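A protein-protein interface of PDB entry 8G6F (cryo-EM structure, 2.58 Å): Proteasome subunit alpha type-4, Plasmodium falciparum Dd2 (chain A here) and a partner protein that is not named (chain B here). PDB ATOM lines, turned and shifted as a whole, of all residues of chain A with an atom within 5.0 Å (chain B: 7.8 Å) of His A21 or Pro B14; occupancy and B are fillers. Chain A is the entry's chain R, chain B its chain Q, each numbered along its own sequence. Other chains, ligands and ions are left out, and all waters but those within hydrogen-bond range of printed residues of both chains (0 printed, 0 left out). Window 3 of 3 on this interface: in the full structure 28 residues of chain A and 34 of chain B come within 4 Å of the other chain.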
ATOM      1  N   LEU A  17     -25.490  -4.237 -15.821  1.00  0.00           N
ATOM      2  CA  LEU A  17     -24.576  -3.707 -16.824  1.00  0.00           C
ATOM      3  C   LEU A  17     -24.245  -2.246 -16.567  1.00  0.00           C
ATOM      4  O   LEU A  17     -23.130  -1.806 -16.858  1.00  0.00           O
ATOM      5  CB  LEU A  17     -25.173  -3.883 -18.218  1.00  0.00           C
ATOM      6  CG  LEU A  17     -25.344  -5.325 -18.699  1.00  0.00           C
ATOM      7  CD1 LEU A  17     -25.715  -5.349 -20.166  1.00  0.00           C
ATOM      8  CD2 LEU A  17     -24.094  -6.153 -18.458  1.00  0.00           C
ATOM      9  N   GLN A  18     -25.190  -1.477 -16.029  1.00  0.00           N
ATOM     10  CA  GLN A  18     -24.888  -0.094 -15.687  1.00  0.00           C
ATOM     11  C   GLN A  18     -23.785  -0.025 -14.641  1.00  0.00           C
ATOM     12  O   GLN A  18     -22.903   0.838 -14.709  1.00  0.00           O
ATOM     13  CB  GLN A  18     -26.146   0.611 -15.188  1.00  0.00           C
ATOM     14  CG  GLN A  18     -27.153   0.906 -16.277  1.00  0.00           C
ATOM     15  CD  GLN A  18     -26.665   1.947 -17.251  1.00  0.00           C
ATOM     16  OE1 GLN A  18     -26.682   3.139 -16.959  1.00  0.00           O
ATOM     17  NE2 GLN A  18     -26.226   1.505 -18.419  1.00  0.00           N
ATOM     18  N   VAL A  19     -23.817  -0.930 -13.664  1.00  0.00           N
ATOM     19  CA  VAL A  19     -22.775  -0.959 -12.647  1.00  0.00           C
ATOM     20  C   VAL A  19     -21.446  -1.380 -13.259  1.00  0.00           C
ATOM     21  O   VAL A  19     -20.387  -0.846 -12.907  1.00  0.00           O
ATOM     22  CB  VAL A  19     -23.193  -1.884 -11.493  1.00  0.00           C
ATOM     23  CG1 VAL A  19     -22.101  -1.958 -10.448  1.00  0.00           C
ATOM     24  CG2 VAL A  19     -24.488  -1.395 -10.878  1.00  0.00           C
ATOM     25  N   GLU A  20     -21.474  -2.336 -14.187  1.00  0.00           N
ATOM     26  CA  GLU A  20     -20.236  -2.703 -14.871  1.00  0.00           C
ATOM     27  C   GLU A  20     -19.656  -1.514 -15.630  1.00  0.00           C
ATOM     28  O   GLU A  20     -18.440  -1.299 -15.631  1.00  0.00           O
ATOM     29  CB  GLU A  20     -20.473  -3.876 -15.823  1.00  0.00           C
ATOM     30  CG  GLU A  20     -21.363  -4.977 -15.282  1.00  0.00           C
ATOM     31  CD  GLU A  20     -21.015  -5.385 -13.867  1.00  0.00           C
ATOM     32  OE1 GLU A  20     -19.863  -5.160 -13.444  1.00  0.00           O
ATOM     33  OE2 GLU A  20     -21.897  -5.934 -13.174  1.00  0.00           O
ATOM     34  N   HIS A  21     -20.514  -0.728 -16.280  1.00  0.00           N
ATOM     35  CA  HIS A  21     -20.039   0.434 -17.026  1.00  0.00           C
ATOM     36  C   HIS A  21     -19.507   1.514 -16.092  1.00  0.00           C
ATOM     37  O   HIS A  21     -18.547   2.220 -16.427  1.00  0.00           O
ATOM     38  CB  HIS A  21     -21.163   0.981 -17.900  1.00  0.00           C
ATOM     39  CG  HIS A  21     -21.792  -0.049 -18.784  1.00  0.00           C
ATOM     40  ND1 HIS A  21     -23.061   0.088 -19.301  1.00  0.00           N
ATOM     41  CD2 HIS A  21     -21.328  -1.237 -19.239  1.00  0.00           C
ATOM     42  CE1 HIS A  21     -23.350  -0.968 -20.039  1.00  0.00           C
ATOM     43  NE2 HIS A  21     -22.315  -1.787 -20.019  1.00  0.00           N
ATOM     44  N   ALA A  22     -20.117   1.666 -14.918  1.00  0.00           N
ATOM     45  CA  ALA A  22     -19.561   2.577 -13.924  1.00  0.00           C
ATOM     46  C   ALA A  22     -18.173   2.120 -13.491  1.00  0.00           C
ATOM     47  O   ALA A  22     -17.265   2.939 -13.305  1.00  0.00           O
ATOM     48  CB  ALA A  22     -20.500   2.681 -12.724  1.00  0.00           C
ATOM     49  N   LEU A  23     -17.988   0.808 -13.338  1.00  0.00           N
ATOM     50  CA  LEU A  23     -16.658   0.288 -13.034  1.00  0.00           C
ATOM     51  C   LEU A  23     -15.681   0.581 -14.165  1.00  0.00           C
ATOM     52  O   LEU A  23     -14.501   0.856 -13.922  1.00  0.00           O
ATOM     53  CB  LEU A  23     -16.730  -1.214 -12.771  1.00  0.00           C
ATOM     54  CG  LEU A  23     -17.271  -1.622 -11.404  1.00  0.00           C
ATOM     55  CD1 LEU A  23     -17.770  -3.050 -11.446  1.00  0.00           C
ATOM     56  CD2 LEU A  23     -16.204  -1.456 -10.342  1.00  0.00           C
ATOM     57  N   GLU A  24     -16.145   0.504 -15.412  1.00  0.00           N
ATOM     58  CA  GLU A  24     -15.272   0.825 -16.538  1.00  0.00           C
ATOM     59  C   GLU A  24     -14.857   2.290 -16.513  1.00  0.00           C
ATOM     60  O   GLU A  24     -13.706   2.626 -16.816  1.00  0.00           O
ATOM     61  CB  GLU A  24     -15.963   0.486 -17.858  1.00  0.00           C
ATOM     62  CG  GLU A  24     -16.240  -0.992 -18.051  1.00  0.00           C
ATOM     63  CD  GLU A  24     -15.028  -1.857 -17.769  1.00  0.00           C
ATOM     64  OE1 GLU A  24     -13.949  -1.573 -18.333  1.00  0.00           O
ATOM     65  OE2 GLU A  24     -15.152  -2.813 -16.974  1.00  0.00           O
ATOM     66  N   ALA A  25     -15.783   3.180 -16.160  1.00  0.00           N
ATOM     67  CA  ALA A  25     -15.419   4.584 -15.991  1.00  0.00           C
ATOM     68  C   ALA A  25     -14.388   4.748 -14.880  1.00  0.00           C
ATOM     69  O   ALA A  25     -13.441   5.535 -15.003  1.00  0.00           O
ATOM     70  CB  ALA A  25     -16.662   5.421 -15.693  1.00  0.00           C
ATOM     71  N   THR B  11     -27.528   7.553 -19.447  1.00  0.00           N
ATOM     72  CA  THR B  11     -27.234   6.135 -19.323  1.00  0.00           C
ATOM     73  C   THR B  11     -25.794   5.878 -19.738  1.00  0.00           C
ATOM     74  O   THR B  11     -25.295   6.486 -20.688  1.00  0.00           O
ATOM     75  CB  THR B  11     -28.193   5.300 -20.181  1.00  0.00           C
ATOM     76  OG1 THR B  11     -29.503   5.340 -19.605  1.00  0.00           O
ATOM     77  CG2 THR B  11     -27.731   3.864 -20.268  1.00  0.00           C
ATOM     78  N   PHE B  12     -25.130   4.982 -19.015  1.00  0.00           N
ATOM     79  CA  PHE B  12     -23.759   4.619 -19.342  1.00  0.00           C
ATOM     80  C   PHE B  12     -23.718   3.760 -20.599  1.00  0.00           C
ATOM     81  O   PHE B  12     -24.682   3.073 -20.944  1.00  0.00           O
ATOM     82  CB  PHE B  12     -23.117   3.852 -18.188  1.00  0.00           C
ATOM     83  CG  PHE B  12     -22.490   4.725 -17.144  1.00  0.00           C
ATOM     84  CD1 PHE B  12     -21.409   5.528 -17.448  1.00  0.00           C
ATOM     85  CD2 PHE B  12     -22.975   4.728 -15.848  1.00  0.00           C
ATOM     86  CE1 PHE B  12     -20.830   6.324 -16.482  1.00  0.00           C
ATOM     87  CE2 PHE B  12     -22.400   5.521 -14.881  1.00  0.00           C
ATOM     88  CZ  PHE B  12     -21.327   6.320 -15.199  1.00  0.00           C
ATOM     89  N   SER B  13     -22.589   3.799 -21.275  1.00  0.00           N
ATOM     90  CA  SER B  13     -22.308   2.961 -22.426  1.00  0.00           C
ATOM     91  C   SER B  13     -21.366   1.836 -22.036  1.00  0.00           C
ATOM     92  O   SER B  13     -20.810   1.823 -20.935  1.00  0.00           O
ATOM     93  CB  SER B  13     -21.703   3.808 -23.546  1.00  0.00           C
ATOM     94  OG  SER B  13     -22.695   4.624 -24.140  1.00  0.00           O
ATOM     95  N   PRO B  14     -21.155   0.860 -22.922  1.00  0.00           N
ATOM     96  CA  PRO B  14     -20.294  -0.275 -22.557  1.00  0.00           C
ATOM     97  C   PRO B  14     -18.897   0.126 -22.120  1.00  0.00           C
ATOM     98  O   PRO B  14     -18.293  -0.575 -21.300  1.00  0.00           O
ATOM     99  CB  PRO B  14     -20.270  -1.111 -23.840  1.00  0.00           C
ATOM    100  CG  PRO B  14     -21.568  -0.822 -24.483  1.00  0.00           C
ATOM    101  CD  PRO B  14     -21.858   0.620 -24.193  1.00  0.00           C
ATOM    102  N   GLU B  15     -18.359   1.221 -22.642  1.00  0.00           N
ATOM    103  CA  GLU B  15     -17.029   1.673 -22.260  1.00  0.00           C
ATOM    104  C   GLU B  15     -17.047   2.604 -21.056  1.00  0.00           C
ATOM    105  O   GLU B  15     -15.988   3.093 -20.656  1.00  0.00           O
ATOM    106  CB  GLU B  15     -16.353   2.373 -23.439  1.00  0.00           C
ATOM    107  CG  GLU B  15     -15.961   1.447 -24.580  1.00  0.00           C
ATOM    108  CD  GLU B  15     -16.888   1.562 -25.777  1.00  0.00           C
ATOM    109  OE1 GLU B  15     -18.047   1.992 -25.601  1.00  0.00           O
ATOM    110  OE2 GLU B  15     -16.452   1.233 -26.899  1.00  0.00           O
ATOM    111  N   GLY B  16     -18.213   2.864 -20.476  1.00  0.00           N
ATOM    112  CA  GLY B  16     -18.297   3.703 -19.301  1.00  0.00           C
ATOM    113  C   GLY B  16     -18.257   5.178 -19.630  1.00  0.00           C
ATOM    114  O   GLY B  16     -17.515   5.940 -19.006  1.00  0.00           O
ATOM    115  N   ARG B  17     -19.051   5.594 -20.613  1.00  0.00           N
ATOM    116  CA  ARG B  17     -19.106   6.990 -21.016  1.00  0.00           C
ATOM    117  C   ARG B  17     -20.526   7.318 -21.446  1.00  0.00           C
ATOM    118  O   ARG B  17     -21.367   6.432 -21.605  1.00  0.00           O
ATOM    119  CB  ARG B  17     -18.114   7.284 -22.141  1.00  0.00           C
ATOM    120  CG  ARG B  17     -18.351   6.469 -23.391  1.00  0.00           C
ATOM    121  CD  ARG B  17     -17.091   5.767 -23.838  1.00  0.00           C
ATOM    122  NE  ARG B  17     -17.269   5.119 -25.132  1.00  0.00           N
ATOM    123  CZ  ARG B  17     -17.073   5.710 -26.303  1.00  0.00           C
ATOM    124  NH1 ARG B  17     -16.678   6.969 -26.387  1.00  0.00           N
ATOM    125  NH2 ARG B  17     -17.277   5.018 -27.419  1.00  0.00           N
ATOM    126  N   TYR B  19     -22.849   8.956 -24.269  1.00  0.00           N
ATOM    127  CA  TYR B  19     -22.872   9.328 -25.679  1.00  0.00           C
ATOM    128  C   TYR B  19     -23.387  10.746 -25.868  1.00  0.00           C
ATOM    129  O   TYR B  19     -22.896  11.481 -26.729  1.00  0.00           O
ATOM    130  CB  TYR B  19     -23.741   8.349 -26.464  1.00  0.00           C
ATOM    131  CG  TYR B  19     -23.124   6.994 -26.726  1.00  0.00           C
ATOM    132  CD1 TYR B  19     -21.750   6.829 -26.812  1.00  0.00           C
ATOM    133  CD2 TYR B  19     -23.926   5.879 -26.904  1.00  0.00           C
ATOM    134  CE1 TYR B  19     -21.196   5.592 -27.059  1.00  0.00           C
ATOM    135  CE2 TYR B  19     -23.379   4.639 -27.150  1.00  0.00           C
ATOM    136  CZ  TYR B  19     -22.016   4.501 -27.226  1.00  0.00           C
ATOM    137  OH  TYR B  19     -21.472   3.264 -27.472  1.00  0.00           O
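O of Ser B13 sits close to ND1 of His A21 (3.3 Å). OE1 of Gln A18 is in hydrogen-bond range of N of Phe B12.
The guanidinium group (NE) of Arg B17 lies within salt-bridge range of the side-chain carboxylate (OE1) of Glu B15 (3.3 Å). O of Arg B17 lies close to OG of Ser B13. The backbone carbonyl oxygen of Leu A17 lies close to a ring nitrogen (ND1) of His A21 (3.1 Å).
Gln A18 touches Thr B11 (NE2 to CG2, 3.4 Å). His A21 touches Phe B12 (CB to CB, 3.5 Å). Pro B14 touches His A21. His A21 touches Gly B16 (O to CA, 3.2 Å). CG of Glu A24 touches O of Pro B14, at 3.9 Å. Glu B15 touches Glu A24 (O to CB, 3.8 Å). CB of Ala A25 touches O of Gly B16, 3.5 Å away.
Printed residues of chain B within 4 Å of Gln A18: Thr B11 and Phe B12. Val A19 touches none of the printed residues of chain B. His A21 touches just these residues of chain B: Phe B12 (3.5 Å), Ser B13 (3.0 Å), Pro B14 (3.6 Å) and Gly B16 (3.2 Å). Of the printed residues of chain B, Glu A24 touches Pro B14 and Glu B15. Printed residues of chain B within 4 Å of Ala A25: Gly B16. Of the printed residues of chain A, Phe B12 touches Gln A18 (3.2 Å) and His A21 (3.5 Å). Of the printed residues of chain A, Ser B13 touches His A21. The nearest printed residue of chain A that does not touch Pro B14 is Glu A20 (5.7 Å). The nearest printed residue of chain A that does not touch Glu B15 is Ala A25 (4.5 Å).
Of the 8 printed residues of chain B, 6 touch a printed residue of chain A. Printed residues of chain B that touch a printed residue of chain A: Thr B11, Phe B12, Ser B13, Pro B14, Glu B15 and Gly B16. Hydrophobic or aromatic side chains of chain B within 4 Å of the printed part of chain A: Phe B12. Printed residues of chain A that touch a printed residue of chain B: Gln A18, His A21, Glu A24 and Ala A25. Hydrophobic or aromatic side chains of chain A within 4 Å of the printed part of chain B: His A21 and Ala A25. Among the printed residues, no Asp or Glu carboxylate lies within 4 Å of a Lys or Arg side-chain nitrogen of the other chain.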
